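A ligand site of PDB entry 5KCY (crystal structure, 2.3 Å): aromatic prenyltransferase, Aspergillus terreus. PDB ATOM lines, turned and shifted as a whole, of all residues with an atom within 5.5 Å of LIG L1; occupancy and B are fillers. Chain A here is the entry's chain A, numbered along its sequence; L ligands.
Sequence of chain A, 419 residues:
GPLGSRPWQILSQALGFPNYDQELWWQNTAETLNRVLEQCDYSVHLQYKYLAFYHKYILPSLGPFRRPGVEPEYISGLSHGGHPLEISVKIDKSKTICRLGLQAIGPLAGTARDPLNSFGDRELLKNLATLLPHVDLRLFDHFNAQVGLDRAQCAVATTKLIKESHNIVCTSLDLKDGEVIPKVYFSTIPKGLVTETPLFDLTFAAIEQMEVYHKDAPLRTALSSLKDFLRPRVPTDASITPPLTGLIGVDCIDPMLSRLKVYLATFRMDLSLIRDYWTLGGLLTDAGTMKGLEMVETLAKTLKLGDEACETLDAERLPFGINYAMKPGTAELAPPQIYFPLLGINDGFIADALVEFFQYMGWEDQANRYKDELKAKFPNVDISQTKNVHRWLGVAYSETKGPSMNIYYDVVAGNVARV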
ATOM      1  N   HIS A  83     -18.515   3.179  -9.617  1.00  0.00           N
ATOM      2  CA  HIS A  83     -19.662   3.669 -10.356  1.00  0.00           C
ATOM      3  C   HIS A  83     -20.246   4.969  -9.753  1.00  0.00           C
ATOM      4  O   HIS A  83     -20.077   5.261  -8.581  1.00  0.00           O
ATOM      5  CB  HIS A  83     -20.712   2.579 -10.500  1.00  0.00           C
ATOM      6  CG  HIS A  83     -21.651   2.415  -9.336  1.00  0.00           C
ATOM      7  ND1 HIS A  83     -22.701   3.266  -9.094  1.00  0.00           N
ATOM      8  CD2 HIS A  83     -21.747   1.444  -8.386  1.00  0.00           C
ATOM      9  CE1 HIS A  83     -23.381   2.868  -8.032  1.00  0.00           C
ATOM     10  NE2 HIS A  83     -22.810   1.766  -7.579  1.00  0.00           N
ATOM     11  N   PRO A  84     -20.879   5.792 -10.590  1.00  0.00           N
ATOM     12  CA  PRO A  84     -21.345   7.095 -10.073  1.00  0.00           C
ATOM     13  C   PRO A  84     -22.566   6.941  -9.117  1.00  0.00           C
ATOM     14  O   PRO A  84     -23.286   5.968  -9.206  1.00  0.00           O
ATOM     15  CB  PRO A  84     -21.724   7.890 -11.350  1.00  0.00           C
ATOM     16  CG  PRO A  84     -21.522   6.934 -12.508  1.00  0.00           C
ATOM     17  CD  PRO A  84     -21.323   5.545 -11.973  1.00  0.00           C
ATOM     18  N   GLU A  86     -25.892   6.776  -7.967  1.00  0.00           N
ATOM     19  CA  GLU A  86     -27.061   6.534  -8.739  1.00  0.00           C
ATOM     20  C   GLU A  86     -28.312   6.690  -7.885  1.00  0.00           C
ATOM     21  O   GLU A  86     -28.376   6.242  -6.754  1.00  0.00           O
ATOM     22  CB  GLU A  86     -26.945   5.141  -9.374  1.00  0.00           C
ATOM     23  CG  GLU A  86     -26.008   5.203 -10.583  1.00  0.00           C
ATOM     24  CD  GLU A  86     -25.727   3.862 -11.198  1.00  0.00           C
ATOM     25  OE1 GLU A  86     -26.699   3.146 -11.476  1.00  0.00           O
ATOM     26  OE2 GLU A  86     -24.549   3.512 -11.403  1.00  0.00           O
ATOM     27  N   GLY A 101     -27.787   4.076  -4.931  1.00  0.00           N
ATOM     28  CA  GLY A 101     -26.774   3.106  -5.258  1.00  0.00           C
ATOM     29  C   GLY A 101     -25.451   3.843  -5.221  1.00  0.00           C
ATOM     30  O   GLY A 101     -25.304   4.916  -5.862  1.00  0.00           O
ATOM     31  N   CYS A 170     -20.055  -2.725  -3.748  1.00  0.00           N
ATOM     32  CA  CYS A 170     -20.823  -1.541  -3.645  1.00  0.00           C
ATOM     33  C   CYS A 170     -22.155  -1.785  -2.999  1.00  0.00           C
ATOM     34  O   CYS A 170     -22.486  -2.889  -2.617  1.00  0.00           O
ATOM     35  CB  CYS A 170     -20.886  -0.859  -4.977  1.00  0.00           C
ATOM     36  SG  CYS A 170     -21.634  -1.830  -6.198  1.00  0.00           S
ATOM     37  N   THR A 171     -22.872  -0.724  -2.753  1.00  0.00           N
ATOM     38  CA  THR A 171     -23.984  -0.764  -1.833  1.00  0.00           C
ATOM     39  C   THR A 171     -25.188  -0.066  -2.409  1.00  0.00           C
ATOM     40  O   THR A 171     -25.040   0.933  -3.041  1.00  0.00           O
ATOM     41  CB  THR A 171     -23.592  -0.033  -0.515  1.00  0.00           C
ATOM     42  OG1 THR A 171     -22.397  -0.580   0.027  1.00  0.00           O
ATOM     43  CG2 THR A 171     -24.664  -0.190   0.518  1.00  0.00           C
ATOM     44  N   SER A 172     -26.389  -0.524  -2.097  1.00  0.00           N
ATOM     45  CA  SER A 172     -27.637   0.191  -2.405  1.00  0.00           C
ATOM     46  C   SER A 172     -28.524   0.263  -1.186  1.00  0.00           C
ATOM     47  O   SER A 172     -28.563  -0.638  -0.355  1.00  0.00           O
ATOM     48  CB  SER A 172     -28.460  -0.575  -3.476  1.00  0.00           C
ATOM     49  OG  SER A 172     -28.041  -0.120  -4.745  1.00  0.00           O
ATOM     50  N   TYR A 185     -23.250  -5.636  -3.348  1.00  0.00           N
ATOM     51  CA  TYR A 185     -22.868  -6.288  -4.602  1.00  0.00           C
ATOM     52  C   TYR A 185     -21.382  -6.529  -4.553  1.00  0.00           C
ATOM     53  O   TYR A 185     -20.598  -5.614  -4.230  1.00  0.00           O
ATOM     54  CB  TYR A 185     -23.232  -5.377  -5.793  1.00  0.00           C
ATOM     55  CG  TYR A 185     -24.647  -4.818  -5.710  1.00  0.00           C
ATOM     56  CD1 TYR A 185     -24.900  -3.674  -4.970  1.00  0.00           C
ATOM     57  CD2 TYR A 185     -25.701  -5.409  -6.382  1.00  0.00           C
ATOM     58  CE1 TYR A 185     -26.182  -3.152  -4.861  1.00  0.00           C
ATOM     59  CE2 TYR A 185     -26.987  -4.903  -6.313  1.00  0.00           C
ATOM     60  CZ  TYR A 185     -27.229  -3.765  -5.541  1.00  0.00           C
ATOM     61  OH  TYR A 185     -28.515  -3.251  -5.426  1.00  0.00           O
ATOM     62  N   SER A 187     -18.078  -7.863  -6.598  1.00  0.00           N
ATOM     63  CA  SER A 187     -17.486  -8.258  -7.907  1.00  0.00           C
ATOM     64  C   SER A 187     -16.607  -9.416  -7.712  1.00  0.00           C
ATOM     65  O   SER A 187     -15.817  -9.471  -6.758  1.00  0.00           O
ATOM     66  CB  SER A 187     -16.629  -7.199  -8.568  1.00  0.00           C
ATOM     67  OG  SER A 187     -17.294  -5.946  -8.476  1.00  0.00           O
ATOM     68  N   ILE A 189     -14.615 -10.319 -10.406  1.00  0.00           N
ATOM     69  CA  ILE A 189     -13.517 -10.185 -11.352  1.00  0.00           C
ATOM     70  C   ILE A 189     -12.131 -10.093 -10.650  1.00  0.00           C
ATOM     71  O   ILE A 189     -11.207 -10.825 -10.998  1.00  0.00           O
ATOM     72  CB  ILE A 189     -13.793  -9.061 -12.362  1.00  0.00           C
ATOM     73  CG1 ILE A 189     -15.013  -9.476 -13.177  1.00  0.00           C
ATOM     74  CG2 ILE A 189     -12.524  -8.757 -13.205  1.00  0.00           C
ATOM     75  CD1 ILE A 189     -15.418  -8.537 -14.303  1.00  0.00           C
ATOM     76  N   LEU A 244     -20.583 -13.136 -18.726  1.00  0.00           N
ATOM     77  CA  LEU A 244     -19.914 -13.642 -17.538  1.00  0.00           C
ATOM     78  C   LEU A 244     -20.646 -13.319 -16.243  1.00  0.00           C
ATOM     79  O   LEU A 244     -21.395 -12.353 -16.167  1.00  0.00           O
ATOM     80  CB  LEU A 244     -18.497 -13.085 -17.490  1.00  0.00           C
ATOM     81  CG  LEU A 244     -18.290 -11.574 -17.515  1.00  0.00           C
ATOM     82  CD1 LEU A 244     -18.556 -10.951 -16.164  1.00  0.00           C
ATOM     83  CD2 LEU A 244     -16.854 -11.252 -17.920  1.00  0.00           C
ATOM     84  N   GLY A 246     -20.409 -11.668 -13.242  1.00  0.00           N
ATOM     85  CA  GLY A 246     -19.579 -10.556 -12.716  1.00  0.00           C
ATOM     86  C   GLY A 246     -19.919  -9.977 -11.360  1.00  0.00           C
ATOM     87  O   GLY A 246     -19.106  -9.247 -10.779  1.00  0.00           O
ATOM     88  N   LEU A 247     -21.091 -10.303 -10.831  1.00  0.00           N
ATOM     89  CA  LEU A 247     -21.579  -9.709  -9.587  1.00  0.00           C
ATOM     90  C   LEU A 247     -22.451 -10.671  -8.864  1.00  0.00           C
ATOM     91  O   LEU A 247     -23.346 -11.273  -9.464  1.00  0.00           O
ATOM     92  CB  LEU A 247     -22.455  -8.521  -9.845  1.00  0.00           C
ATOM     93  CG  LEU A 247     -22.088  -7.082  -9.736  1.00  0.00           C
ATOM     94  CD1 LEU A 247     -23.394  -6.309  -9.681  1.00  0.00           C
ATOM     95  CD2 LEU A 247     -21.153  -6.712  -8.592  1.00  0.00           C
ATOM     96  N   ALA A 265     -22.989 -10.083 -17.067  1.00  0.00           N
ATOM     97  CA  ALA A 265     -22.677  -8.942 -17.922  1.00  0.00           C
ATOM     98  C   ALA A 265     -22.329  -9.425 -19.305  1.00  0.00           C
ATOM     99  O   ALA A 265     -21.575 -10.360 -19.458  1.00  0.00           O
ATOM    100  CB  ALA A 265     -21.518  -8.134 -17.344  1.00  0.00           C
ATOM    101  N   LEU A 318     -21.595   0.443 -22.007  1.00  0.00           N
ATOM    102  CA  LEU A 318     -21.665  -0.484 -20.871  1.00  0.00           C
ATOM    103  C   LEU A 318     -22.307  -1.789 -21.317  1.00  0.00           C
ATOM    104  O   LEU A 318     -22.994  -1.835 -22.310  1.00  0.00           O
ATOM    105  CB  LEU A 318     -22.532   0.112 -19.797  1.00  0.00           C
ATOM    106  CG  LEU A 318     -22.033   1.385 -19.113  1.00  0.00           C
ATOM    107  CD1 LEU A 318     -23.219   2.056 -18.460  1.00  0.00           C
ATOM    108  CD2 LEU A 318     -20.987   1.044 -18.089  1.00  0.00           C
ATOM    109  N   PRO A 319     -22.065  -2.863 -20.584  1.00  0.00           N
ATOM    110  CA  PRO A 319     -22.703  -4.076 -20.963  1.00  0.00           C
ATOM    111  C   PRO A 319     -24.191  -4.116 -20.638  1.00  0.00           C
ATOM    112  O   PRO A 319     -24.686  -3.336 -19.860  1.00  0.00           O
ATOM    113  CB  PRO A 319     -21.913  -5.129 -20.159  1.00  0.00           C
ATOM    114  CG  PRO A 319     -21.275  -4.414 -19.033  1.00  0.00           C
ATOM    115  CD  PRO A 319     -21.081  -3.032 -19.497  1.00  0.00           C
ATOM    116  N   ARG A 391     -28.939   6.064 -17.001  1.00  0.00           N
ATOM    117  CA  ARG A 391     -27.853   5.120 -17.137  1.00  0.00           C
ATOM    118  C   ARG A 391     -28.276   3.718 -17.450  1.00  0.00           C
ATOM    119  O   ARG A 391     -27.628   3.040 -18.237  1.00  0.00           O
ATOM    120  CB  ARG A 391     -27.006   5.150 -15.874  1.00  0.00           C
ATOM    121  CG  ARG A 391     -25.630   4.553 -16.044  1.00  0.00           C
ATOM    122  CD  ARG A 391     -24.837   4.818 -14.770  1.00  0.00           C
ATOM    123  NE  ARG A 391     -23.588   4.085 -14.772  1.00  0.00           N
ATOM    124  CZ  ARG A 391     -22.447   4.510 -15.294  1.00  0.00           C
ATOM    125  NH1 ARG A 391     -22.343   5.665 -15.941  1.00  0.00           N
ATOM    126  NH2 ARG A 391     -21.370   3.753 -15.183  1.00  0.00           N
ATOM    127  N   TRP A 392     -29.293   3.233 -16.766  1.00  0.00           N
ATOM    128  CA  TRP A 392     -29.767   1.865 -16.928  1.00  0.00           C
ATOM    129  C   TRP A 392     -31.233   1.942 -16.919  1.00  0.00           C
ATOM    130  O   TRP A 392     -31.831   2.829 -16.300  1.00  0.00           O
ATOM    131  CB  TRP A 392     -29.399   0.936 -15.774  1.00  0.00           C
ATOM    132  CG  TRP A 392     -27.927   0.778 -15.509  1.00  0.00           C
ATOM    133  CD1 TRP A 392     -27.206   1.390 -14.551  1.00  0.00           C
ATOM    134  CD2 TRP A 392     -27.028  -0.078 -16.197  1.00  0.00           C
ATOM    135  NE1 TRP A 392     -25.901   0.993 -14.593  1.00  0.00           N
ATOM    136  CE2 TRP A 392     -25.751   0.102 -15.613  1.00  0.00           C
ATOM    137  CE3 TRP A 392     -27.158  -0.952 -17.264  1.00  0.00           C
ATOM    138  CZ2 TRP A 392     -24.624  -0.555 -16.062  1.00  0.00           C
ATOM    139  CZ3 TRP A 392     -26.060  -1.651 -17.679  1.00  0.00           C
ATOM    140  CH2 TRP A 392     -24.799  -1.446 -17.091  1.00  0.00           C
ATOM    141  N   TYR A 408     -32.303   4.043 -13.608  1.00  0.00           N
ATOM    142  CA  TYR A 408     -31.158   4.448 -12.881  1.00  0.00           C
ATOM    143  C   TYR A 408     -30.595   5.761 -13.485  1.00  0.00           C
ATOM    144  O   TYR A 408     -30.207   5.781 -14.657  1.00  0.00           O
ATOM    145  CB  TYR A 408     -30.095   3.354 -12.896  1.00  0.00           C
ATOM    146  CG  TYR A 408     -30.526   2.115 -12.161  1.00  0.00           C
ATOM    147  CD1 TYR A 408     -31.487   1.286 -12.709  1.00  0.00           C
ATOM    148  CD2 TYR A 408     -30.034   1.783 -10.869  1.00  0.00           C
ATOM    149  CE1 TYR A 408     -31.963   0.181 -12.050  1.00  0.00           C
ATOM    150  CE2 TYR A 408     -30.492   0.649 -10.185  1.00  0.00           C
ATOM    151  CZ  TYR A 408     -31.460  -0.148 -10.799  1.00  0.00           C
ATOM    152  OH  TYR A 408     -31.979  -1.299 -10.221  1.00  0.00           O
HETATM  153  C1  LIG L   1     -21.666  -5.210 -12.886  1.00  0.00           C
HETATM  154  C2  LIG L   1     -20.761  -6.203 -13.267  1.00  0.00           C
HETATM  155  C3  LIG L   1     -19.952  -6.029 -14.370  1.00  0.00           C
HETATM  156  O1  LIG L   1     -19.129  -7.053 -14.666  1.00  0.00           O
HETATM  157  C4  LIG L   1     -20.052  -4.832 -15.092  1.00  0.00           C
HETATM  158  C5  LIG L   1     -20.955  -3.812 -14.693  1.00  0.00           C
HETATM  159  C6  LIG L   1     -21.772  -3.976 -13.548  1.00  0.00           C
HETATM  160  C7  LIG L   1     -22.723  -3.060 -13.016  1.00  0.00           C
HETATM  161  C8  LIG L   1     -22.109  -1.740 -12.364  1.00  0.00           C
HETATM  162  C9  LIG L   1     -21.112  -1.893 -11.316  1.00  0.00           C
HETATM  163  O2  LIG L   1     -20.348  -0.951 -11.056  1.00  0.00           O
HETATM  164  O3  LIG L   1     -21.030  -3.107 -10.660  1.00  0.00           O
HETATM  165  C10 LIG L   1     -19.791  -3.306  -9.896  1.00  0.00           C
HETATM  166  O4  LIG L   1     -21.415  -1.099 -13.469  1.00  0.00           O
HETATM  167  C11 LIG L   1     -21.956   0.122 -13.603  1.00  0.00           C
HETATM  168  O5  LIG L   1     -21.574   0.928 -14.451  1.00  0.00           O
HETATM  169  C12 LIG L   1     -22.946   0.370 -12.730  1.00  0.00           C
HETATM  170  O6  LIG L   1     -23.603   1.587 -12.830  1.00  0.00           O
HETATM  171  C13 LIG L   1     -23.158  -0.744 -11.956  1.00  0.00           C
HETATM  172  C14 LIG L   1     -24.070  -0.801 -10.879  1.00  0.00           C
HETATM  173  C15 LIG L   1     -25.102   0.138 -10.670  1.00  0.00           C
HETATM  174  C16 LIG L   1     -25.951   0.129  -9.550  1.00  0.00           C
HETATM  175  C17 LIG L   1     -25.805  -0.850  -8.564  1.00  0.00           C
HETATM  176  O7  LIG L   1     -26.600  -0.907  -7.492  1.00  0.00           O
HETATM  177  C18 LIG L   1     -24.804  -1.806  -8.710  1.00  0.00           C
HETATM  178  C19 LIG L   1     -23.965  -1.758  -9.837  1.00  0.00           C
HETATM  179  P1  LG2 L   2     -33.330  -5.292  -7.666  1.00  0.00           P
HETATM  180  O1  LG2 L   2     -34.686  -5.056  -8.482  1.00  0.00           O
HETATM  181  O2  LG2 L   2     -32.559  -6.476  -8.275  1.00  0.00           O
HETATM  182  O3  LG2 L   2     -33.705  -5.546  -6.222  1.00  0.00           O
HETATM  183  O4  LG2 L   2     -32.494  -4.091  -8.160  1.00  0.00           O
HETATM  184  P2  LG2 L   2     -30.909  -3.822  -7.992  1.00  0.00           P
HETATM  185  O5  LG2 L   2     -30.252  -4.440  -6.817  1.00  0.00           O
HETATM  186  O6  LG2 L   2     -30.908  -2.111  -7.859  1.00  0.00           O
HETATM  187  S1  LG2 L   2     -29.931  -4.282  -9.834  1.00  0.00           S
HETATM  188  C1  LG2 L   2     -28.958  -2.719  -9.748  1.00  0.00           C
HETATM  189  C2  LG2 L   2     -28.566  -2.465 -11.216  1.00  0.00           C
HETATM  190  C3  LG2 L   2     -27.283  -2.976 -11.735  1.00  0.00           C
HETATM  191  C4  LG2 L   2     -26.416  -3.777 -10.759  1.00  0.00           C
HETATM  192  C5  LG2 L   2     -26.902  -2.808 -13.199  1.00  0.00           C
HETATM  193  C6  LG2 L   2     -26.750  -4.261 -13.652  1.00  0.00           C
HETATM  194  C7  LG2 L   2     -25.806  -4.283 -14.844  1.00  0.00           C
HETATM  195  C8  LG2 L   2     -24.845  -5.435 -15.089  1.00  0.00           C
HETATM  196  C9  LG2 L   2     -24.635  -6.536 -14.051  1.00  0.00           C
HETATM  197  C10 LG2 L   2     -23.991  -5.417 -16.347  1.00  0.00           C
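An oxygen (O6) of LG2 L2 is in hydrogen-bond range of the side-chain hydroxyl (OH) of Tyr 408, 2.7 Å away. The side-chain hydroxyl of Ser 172 sits at hydrogen-bond distance from an oxygen (O7) of LIG L1 (3.2 Å). O5 of LIG L1 sits at hydrogen-bond distance from NH2 of Arg 391. The indole nitrogen of Trp 392 sits at hydrogen-bond distance from an oxygen (O6) of LIG L1 (3.0 Å). The side-chain carboxylate (OE2) of Glu 86 sits at hydrogen-bond distance from an oxygen (O6) of LIG L1, at 2.6 Å. OH of Tyr 185 is in hydrogen-bond range of O5 of LG2 L2.
A ring nitrogen (ND1) of His 83 lies within hydrogen-bond range of the side-chain carboxylate (OE2) of Glu 86. The backbone NH (N) of Arg 391 sits at hydrogen-bond distance from the backbone carbonyl oxygen (O) of Tyr 408. The backbone carbonyl oxygen (O) of Cys 170 is in hydrogen-bond range of the backbone NH (N) of Tyr 185 (2.9 Å). The backbone carbonyl oxygen (O) of Gly 101 lies within hydrogen-bond range of the backbone NH (N) of Glu 86, at 2.9 Å. The backbone carbonyl oxygen (O) of Trp 392 sits at hydrogen-bond distance from the backbone NH (N) of Tyr 408 (3.0 Å). OE2 of Glu 86 is in salt-bridge range of NE of Arg 391 (3.5 Å). The side-chain hydroxyl (OH) of Tyr 185 is in hydrogen-bond range of the side-chain hydroxyl (OG) of Ser 172 (3.2 Å). O of Leu 244 is in hydrogen-bond range of N of Ala 265, 2.9 Å away.
His 83 touches LIG L1. Tyr 185 touches LIG L1. Ser 187 touches LIG L1 (OG to C10, 3.9 Å). Leu 247 touches LIG L1. CB of Ala 265 touches O1 of LIG L1, 3.7 Å away. CD2 of Leu 318 touches O5 of LIG L1 (3.7 Å). Hydrophobic or aromatic side chains within 4 Å of LIG L1: His 83, Tyr 185, Leu 247, Ala 265, Leu 318 and Trp 392. Ten residues have an atom within 4 Å of LIG L1: His 83, Glu 86, Ser 172, Tyr 185, Ser 187, Leu 247, Ala 265, Leu 318, Arg 391 and Trp 392.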
